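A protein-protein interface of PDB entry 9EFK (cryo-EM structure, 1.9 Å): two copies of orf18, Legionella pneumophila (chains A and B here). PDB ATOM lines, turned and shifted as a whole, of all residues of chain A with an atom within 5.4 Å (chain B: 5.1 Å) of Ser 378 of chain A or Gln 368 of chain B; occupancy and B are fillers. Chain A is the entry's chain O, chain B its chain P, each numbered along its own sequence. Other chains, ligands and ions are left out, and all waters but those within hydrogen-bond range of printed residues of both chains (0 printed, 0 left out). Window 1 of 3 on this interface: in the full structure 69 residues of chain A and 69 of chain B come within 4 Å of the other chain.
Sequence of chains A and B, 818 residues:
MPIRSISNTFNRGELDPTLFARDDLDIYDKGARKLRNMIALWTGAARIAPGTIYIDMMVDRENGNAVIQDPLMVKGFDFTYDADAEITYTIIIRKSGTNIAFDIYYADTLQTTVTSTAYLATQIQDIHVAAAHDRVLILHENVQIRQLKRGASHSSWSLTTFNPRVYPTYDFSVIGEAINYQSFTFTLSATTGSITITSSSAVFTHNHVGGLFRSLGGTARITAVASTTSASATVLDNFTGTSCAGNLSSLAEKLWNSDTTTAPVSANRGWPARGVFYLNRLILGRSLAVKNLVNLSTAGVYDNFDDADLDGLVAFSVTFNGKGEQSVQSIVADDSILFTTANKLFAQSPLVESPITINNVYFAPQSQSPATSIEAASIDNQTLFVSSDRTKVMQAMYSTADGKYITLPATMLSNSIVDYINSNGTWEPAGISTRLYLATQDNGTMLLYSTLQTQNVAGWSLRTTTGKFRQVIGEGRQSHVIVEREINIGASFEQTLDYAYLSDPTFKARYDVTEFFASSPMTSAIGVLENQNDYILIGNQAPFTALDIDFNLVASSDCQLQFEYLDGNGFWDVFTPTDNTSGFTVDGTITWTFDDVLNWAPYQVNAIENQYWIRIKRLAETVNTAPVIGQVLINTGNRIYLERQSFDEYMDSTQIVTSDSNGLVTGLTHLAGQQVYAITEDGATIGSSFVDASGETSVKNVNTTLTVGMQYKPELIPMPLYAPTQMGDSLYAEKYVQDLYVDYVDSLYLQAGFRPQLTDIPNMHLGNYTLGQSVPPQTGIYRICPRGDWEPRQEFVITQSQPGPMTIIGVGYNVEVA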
ATOM      1  N   VAL A 332      21.846  14.950   6.144  1.00  0.00           N
ATOM      2  CA  VAL A 332      21.334  13.587   6.217  1.00  0.00           C
ATOM      3  C   VAL A 332      22.479  12.617   5.986  1.00  0.00           C
ATOM      4  O   VAL A 332      23.215  12.736   5.000  1.00  0.00           O
ATOM      5  CB  VAL A 332      20.212  13.355   5.193  1.00  0.00           C
ATOM      6  CG1 VAL A 332      19.598  11.984   5.389  1.00  0.00           C
ATOM      7  CG2 VAL A 332      19.163  14.435   5.306  1.00  0.00           C
ATOM      8  N   ASP A 334      22.696   9.592   4.806  1.00  0.00           N
ATOM      9  CA  ASP A 334      22.272   8.516   3.919  1.00  0.00           C
ATOM     10  C   ASP A 334      23.170   8.534   2.695  1.00  0.00           C
ATOM     11  O   ASP A 334      23.381   9.593   2.102  1.00  0.00           O
ATOM     12  CB  ASP A 334      20.807   8.673   3.504  1.00  0.00           C
ATOM     13  CG  ASP A 334      19.840   8.264   4.598  1.00  0.00           C
ATOM     14  OD1 ASP A 334      20.202   7.398   5.423  1.00  0.00           O
ATOM     15  OD2 ASP A 334      18.714   8.804   4.627  1.00  0.00           O
ATOM     16  N   ALA A 376      15.006  15.562   8.407  1.00  0.00           N
ATOM     17  CA  ALA A 376      14.655  14.501   7.475  1.00  0.00           C
ATOM     18  C   ALA A 376      14.714  13.137   8.152  1.00  0.00           C
ATOM     19  O   ALA A 376      15.451  12.924   9.115  1.00  0.00           O
ATOM     20  CB  ALA A 376      15.585  14.520   6.266  1.00  0.00           C
ATOM     21  N   ALA A 377      13.922  12.209   7.630  1.00  0.00           N
ATOM     22  CA  ALA A 377      13.801  10.865   8.168  1.00  0.00           C
ATOM     23  C   ALA A 377      14.370   9.859   7.180  1.00  0.00           C
ATOM     24  O   ALA A 377      14.257  10.037   5.965  1.00  0.00           O
ATOM     25  CB  ALA A 377      12.342  10.530   8.470  1.00  0.00           C
ATOM     26  N   SER A 378      14.992   8.811   7.704  1.00  0.00           N
ATOM     27  CA  SER A 378      15.570   7.749   6.892  1.00  0.00           C
ATOM     28  C   SER A 378      14.884   6.442   7.250  1.00  0.00           C
ATOM     29  O   SER A 378      14.945   6.004   8.402  1.00  0.00           O
ATOM     30  CB  SER A 378      17.077   7.647   7.118  1.00  0.00           C
ATOM     31  OG  SER A 378      17.632   6.586   6.367  1.00  0.00           O
ATOM     32  N   ILE A 379      14.234   5.825   6.268  1.00  0.00           N
ATOM     33  CA  ILE A 379      13.495   4.591   6.503  1.00  0.00           C
ATOM     34  C   ILE A 379      13.165   3.935   5.170  1.00  0.00           C
ATOM     35  O   ILE A 379      12.914   4.625   4.178  1.00  0.00           O
ATOM     36  CB  ILE A 379      12.219   4.866   7.323  1.00  0.00           C
ATOM     37  CG1 ILE A 379      11.498   3.563   7.659  1.00  0.00           C
ATOM     38  CG2 ILE A 379      11.295   5.823   6.587  1.00  0.00           C
ATOM     39  CD1 ILE A 379      10.262   3.753   8.484  1.00  0.00           C
ATOM     40  N   ASP A 380      13.184   2.603   5.136  1.00  0.00           N
ATOM     41  CA  ASP A 380      12.706   1.831   3.988  1.00  0.00           C
ATOM     42  C   ASP A 380      13.420   2.238   2.697  1.00  0.00           C
ATOM     43  O   ASP A 380      12.797   2.487   1.665  1.00  0.00           O
ATOM     44  CB  ASP A 380      11.188   1.963   3.849  1.00  0.00           C
ATOM     45  CG  ASP A 380      10.608   1.030   2.806  1.00  0.00           C
ATOM     46  OD1 ASP A 380      10.691  -0.200   2.987  1.00  0.00           O
ATOM     47  OD2 ASP A 380      10.066   1.530   1.804  1.00  0.00           O
ATOM     48  N   GLN A 382      14.886   4.908   1.703  1.00  0.00           N
ATOM     49  CA  GLN A 382      14.576   6.204   1.119  1.00  0.00           C
ATOM     50  C   GLN A 382      14.726   7.283   2.180  1.00  0.00           C
ATOM     51  O   GLN A 382      14.828   7.001   3.375  1.00  0.00           O
ATOM     52  CB  GLN A 382      13.169   6.225   0.523  1.00  0.00           C
ATOM     53  CG  GLN A 382      12.078   6.051   1.550  1.00  0.00           C
ATOM     54  CD  GLN A 382      10.745   5.708   0.939  1.00  0.00           C
ATOM     55  OE1 GLN A 382      10.252   6.411   0.063  1.00  0.00           O
ATOM     56  NE2 GLN A 382      10.149   4.618   1.399  1.00  0.00           N
ATOM     57  N   THR A 383      14.749   8.530   1.722  1.00  0.00           N
ATOM     58  CA  THR A 383      14.790   9.700   2.586  1.00  0.00           C
ATOM     59  C   THR A 383      13.488  10.472   2.436  1.00  0.00           C
ATOM     60  O   THR A 383      13.058  10.752   1.314  1.00  0.00           O
ATOM     61  CB  THR A 383      15.978  10.599   2.239  1.00  0.00           C
ATOM     62  OG1 THR A 383      17.193   9.848   2.334  1.00  0.00           O
ATOM     63  CG2 THR A 383      16.052  11.775   3.190  1.00  0.00           C
ATOM     64  N   LEU A 384      12.864  10.809   3.560  1.00  0.00           N
ATOM     65  CA  LEU A 384      11.615  11.557   3.586  1.00  0.00           C
ATOM     66  C   LEU A 384      11.829  12.869   4.323  1.00  0.00           C
ATOM     67  O   LEU A 384      12.419  12.882   5.405  1.00  0.00           O
ATOM     68  CB  LEU A 384      10.507  10.747   4.260  1.00  0.00           C
ATOM     69  CG  LEU A 384      10.174   9.418   3.594  1.00  0.00           C
ATOM     70  CD1 LEU A 384       9.144   8.657   4.395  1.00  0.00           C
ATOM     71  CD2 LEU A 384       9.676   9.656   2.187  1.00  0.00           C
ATOM     72  N   THR A 426      10.106   8.329  12.940  1.00  0.00           N
ATOM     73  CA  THR A 426      10.012   7.006  12.340  1.00  0.00           C
ATOM     74  C   THR A 426       9.836   5.961  13.429  1.00  0.00           C
ATOM     75  O   THR A 426      10.146   6.190  14.599  1.00  0.00           O
ATOM     76  CB  THR A 426      11.240   6.667  11.487  1.00  0.00           C
ATOM     77  OG1 THR A 426      12.423   6.752  12.286  1.00  0.00           O
ATOM     78  CG2 THR A 426      11.353   7.615  10.317  1.00  0.00           C
ATOM     79  N   GLU A 428       9.715   1.413  13.729  1.00  0.00           N
ATOM     80  CA  GLU A 428       9.747   0.077  13.145  1.00  0.00           C
ATOM     81  C   GLU A 428       9.361  -0.892  14.252  1.00  0.00           C
ATOM     82  O   GLU A 428      10.219  -1.561  14.839  1.00  0.00           O
ATOM     83  CB  GLU A 428      11.122  -0.232  12.555  1.00  0.00           C
ATOM     84  CG  GLU A 428      11.110  -1.289  11.478  1.00  0.00           C
ATOM     85  CD  GLU A 428      11.997  -0.927  10.302  1.00  0.00           C
ATOM     86  OE1 GLU A 428      12.391   0.253  10.195  1.00  0.00           O
ATOM     87  OE2 GLU A 428      12.298  -1.820   9.484  1.00  0.00           O
ATOM     88  N   ARG A 435       6.630  -0.559   8.303  1.00  0.00           N
ATOM     89  CA  ARG A 435       7.669   0.438   8.530  1.00  0.00           C
ATOM     90  C   ARG A 435       6.998   1.801   8.494  1.00  0.00           C
ATOM     91  O   ARG A 435       6.444   2.190   7.462  1.00  0.00           O
ATOM     92  CB  ARG A 435       8.770   0.349   7.471  1.00  0.00           C
ATOM     93  CG  ARG A 435       9.629  -0.895   7.545  1.00  0.00           C
ATOM     94  CD  ARG A 435      10.513  -1.032   6.314  1.00  0.00           C
ATOM     95  NE  ARG A 435      11.806  -1.617   6.639  1.00  0.00           N
ATOM     96  CZ  ARG A 435      12.722  -1.973   5.748  1.00  0.00           C
ATOM     97  NH1 ARG A 435      12.510  -1.847   4.450  1.00  0.00           N
ATOM     98  NH2 ARG A 435      13.879  -2.468   6.171  1.00  0.00           N
ATOM     99  N   GLU A 475      13.011   7.561  16.338  1.00  0.00           N
ATOM    100  CA  GLU A 475      13.983   7.289  15.287  1.00  0.00           C
ATOM    101  C   GLU A 475      13.980   5.816  14.900  1.00  0.00           C
ATOM    102  O   GLU A 475      14.972   5.298  14.387  1.00  0.00           O
ATOM    103  CB  GLU A 475      15.377   7.739  15.716  1.00  0.00           C
ATOM    104  CG  GLU A 475      15.484   9.237  15.933  1.00  0.00           C
ATOM    105  CD  GLU A 475      16.753   9.633  16.657  1.00  0.00           C
ATOM    106  OE1 GLU A 475      17.730   8.853  16.629  1.00  0.00           O
ATOM    107  OE2 GLU A 475      16.774  10.724  17.264  1.00  0.00           O
ATOM    108  N   ASN B 343      22.160   0.651  14.095  1.00  0.00           N
ATOM    109  CA  ASN B 343      21.223   1.420  13.283  1.00  0.00           C
ATOM    110  C   ASN B 343      21.391   1.185  11.789  1.00  0.00           C
ATOM    111  O   ASN B 343      20.453   0.723  11.137  1.00  0.00           O
ATOM    112  CB  ASN B 343      21.358   2.909  13.610  1.00  0.00           C
ATOM    113  CG  ASN B 343      20.394   3.351  14.676  1.00  0.00           C
ATOM    114  OD1 ASN B 343      19.222   2.995  14.641  1.00  0.00           O
ATOM    115  ND2 ASN B 343      20.878   4.123  15.634  1.00  0.00           N
ATOM    116  N   LYS B 344      22.558   1.460  11.228  1.00  0.00           N
ATOM    117  CA  LYS B 344      22.703   1.576   9.788  1.00  0.00           C
ATOM    118  C   LYS B 344      23.670   0.529   9.256  1.00  0.00           C
ATOM    119  O   LYS B 344      24.580   0.086   9.957  1.00  0.00           O
ATOM    120  CB  LYS B 344      23.179   2.978   9.412  1.00  0.00           C
ATOM    121  CG  LYS B 344      22.548   3.516   8.156  1.00  0.00           C
ATOM    122  CD  LYS B 344      22.514   5.025   8.152  1.00  0.00           C
ATOM    123  CE  LYS B 344      21.570   5.568   9.194  1.00  0.00           C
ATOM    124  NZ  LYS B 344      21.448   7.042   9.075  1.00  0.00           N
ATOM    125  N   GLN B 366      24.621   2.886   4.047  1.00  0.00           N
ATOM    126  CA  GLN B 366      23.545   2.422   3.189  1.00  0.00           C
ATOM    127  C   GLN B 366      22.246   2.481   3.982  1.00  0.00           C
ATOM    128  O   GLN B 366      22.159   3.202   4.979  1.00  0.00           O
ATOM    129  CB  GLN B 366      23.827   1.010   2.675  1.00  0.00           C
ATOM    130  CG  GLN B 366      25.257   0.792   2.203  1.00  0.00           C
ATOM    131  CD  GLN B 366      25.583   1.510   0.911  1.00  0.00           C
ATOM    132  OE1 GLN B 366      25.029   1.201  -0.139  1.00  0.00           O
ATOM    133  NE2 GLN B 366      26.492   2.469   0.981  1.00  0.00           N
ATOM    134  N   SER B 367      21.228   1.757   3.533  1.00  0.00           N
ATOM    135  CA  SER B 367      19.905   1.778   4.148  1.00  0.00           C
ATOM    136  C   SER B 367      19.906   1.655   5.669  1.00  0.00           C
ATOM    137  O   SER B 367      20.833   1.097   6.263  1.00  0.00           O
ATOM    138  CB  SER B 367      19.062   0.653   3.558  1.00  0.00           C
ATOM    139  OG  SER B 367      19.749  -0.576   3.659  1.00  0.00           O
ATOM    140  N   GLN B 368      18.865   2.189   6.301  1.00  0.00           N
ATOM    141  CA  GLN B 368      18.649   2.040   7.733  1.00  0.00           C
ATOM    142  C   GLN B 368      18.121   0.641   8.025  1.00  0.00           C
ATOM    143  O   GLN B 368      17.064   0.255   7.516  1.00  0.00           O
ATOM    144  CB  GLN B 368      17.665   3.101   8.218  1.00  0.00           C
ATOM    145  CG  GLN B 368      17.059   2.832   9.576  1.00  0.00           C
ATOM    146  CD  GLN B 368      17.944   3.295  10.704  1.00  0.00           C
ATOM    147  OE1 GLN B 368      18.970   3.927  10.478  1.00  0.00           O
ATOM    148  NE2 GLN B 368      17.550   2.988  11.930  1.00  0.00           N
ATOM    149  N   SER B 369      18.843  -0.117   8.843  1.00  0.00           N
ATOM    150  CA  SER B 369      18.451  -1.495   9.109  1.00  0.00           C
ATOM    151  C   SER B 369      19.076  -2.002  10.402  1.00  0.00           C
ATOM    152  O   SER B 369      20.134  -2.639  10.368  1.00  0.00           O
ATOM    153  CB  SER B 369      18.856  -2.386   7.938  1.00  0.00           C
ATOM    154  OG  SER B 369      18.262  -3.663   8.043  1.00  0.00           O
ATOM    155  N   PRO B 370      18.460  -1.741  11.553  1.00  0.00           N
ATOM    156  CA  PRO B 370      19.054  -2.169  12.825  1.00  0.00           C
ATOM    157  C   PRO B 370      19.225  -3.678  12.895  1.00  0.00           C
ATOM    158  O   PRO B 370      18.367  -4.441  12.454  1.00  0.00           O
ATOM    159  CB  PRO B 370      18.045  -1.672  13.865  1.00  0.00           C
ATOM    160  CG  PRO B 370      17.342  -0.559  13.197  1.00  0.00           C
ATOM    161  CD  PRO B 370      17.244  -0.942  11.758  1.00  0.00           C
ATOM    162  N   THR B 407      17.836  -3.093   1.831  1.00  0.00           N
ATOM    163  CA  THR B 407      17.434  -4.008   2.887  1.00  0.00           C
ATOM    164  C   THR B 407      15.918  -4.106   2.934  1.00  0.00           C
ATOM    165  O   THR B 407      15.219  -3.092   2.897  1.00  0.00           O
ATOM    166  CB  THR B 407      17.961  -3.566   4.251  1.00  0.00           C
ATOM    167  OG1 THR B 407      17.582  -2.207   4.496  1.00  0.00           O
ATOM    168  CG2 THR B 407      19.468  -3.692   4.308  1.00  0.00           C
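Printed residues of chain B within 4 Å of Asp 334 of chain A: Lys 344. Of the printed residues of chain B, Arg 435 of chain A touches Thr 407 (3.4 Å). Printed residues of chain A within 4 Å of Lys 344 of chain B: Asp 334. Of chain A, only Ser 378 (3.9 Å) comes within 4 Å of Gln 368 of chain B. Pro 370 of chain B touches none of the printed residues of chain A. Printed residues of chain A within 4 Å of Thr 407 of chain B: Arg 435. The nearest residue of chain B that does not touch Ser 378 of chain A is Lys 344 of chain B (4.7 Å).
NZ of Lys 344 of chain B lies within salt-bridge range of OD1 of Asp 334 of chain A, 3.9 Å away. The guanidinium group (NH1) of Arg 435 of chain A lies within hydrogen-bond range of the backbone carbonyl oxygen (O) of Thr 407 of chain B (3.4 Å).
Of the 8 printed residues of chain B, 3 touch a printed residue of chain A. Printed residues of chain B that touch a printed residue of chain A: Lys 344, Gln 368 and Thr 407. Printed residues of chain A that touch a printed residue of chain B: Asp 334, Ser 378 and Arg 435. Along chain A the printed residues that touch a printed residue of chain B span positions 334 to 435. Among the printed residues, Asp or Glu carboxylates within 4 Å of a Lys or Arg side-chain nitrogen of the other chain: Asp 334 of chain A with Lys 344 of chain B (3.9 Å).
Among the printed residues, merely in contact across the chains: Ser 378 of chain A with Gln 368 of chain B (3.9 Å).
The side-chain hydroxyl (OG) of Ser 378 of chain A is in hydrogen-bond range of the side-chain carboxylate (OD1) of Asp 334 of chain A, 2.9 Å away. OD2 of Asp 334 of chain A sits at hydrogen-bond distance from OG1 of Thr 383 of chain A, at 2.9 Å. OD1 of Asp 380 of chain A lies within salt-bridge range of NH1 of Arg 435 of chain A, 2.9 Å away. The side-chain carboxylate of Glu 428 of chain A is in salt-bridge range of the guanidinium group of Arg 435 of chain A, 2.9 Å away. The side-chain amide nitrogen of Gln 368 of chain B sits at hydrogen-bond distance from the side-chain amide oxygen of Asn 343 of chain B (3.2 Å). OG1 of Thr 407 of chain B sits at hydrogen-bond distance from OG of Ser 367 of chain B (2.8 Å).
No position is printed for both chains.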
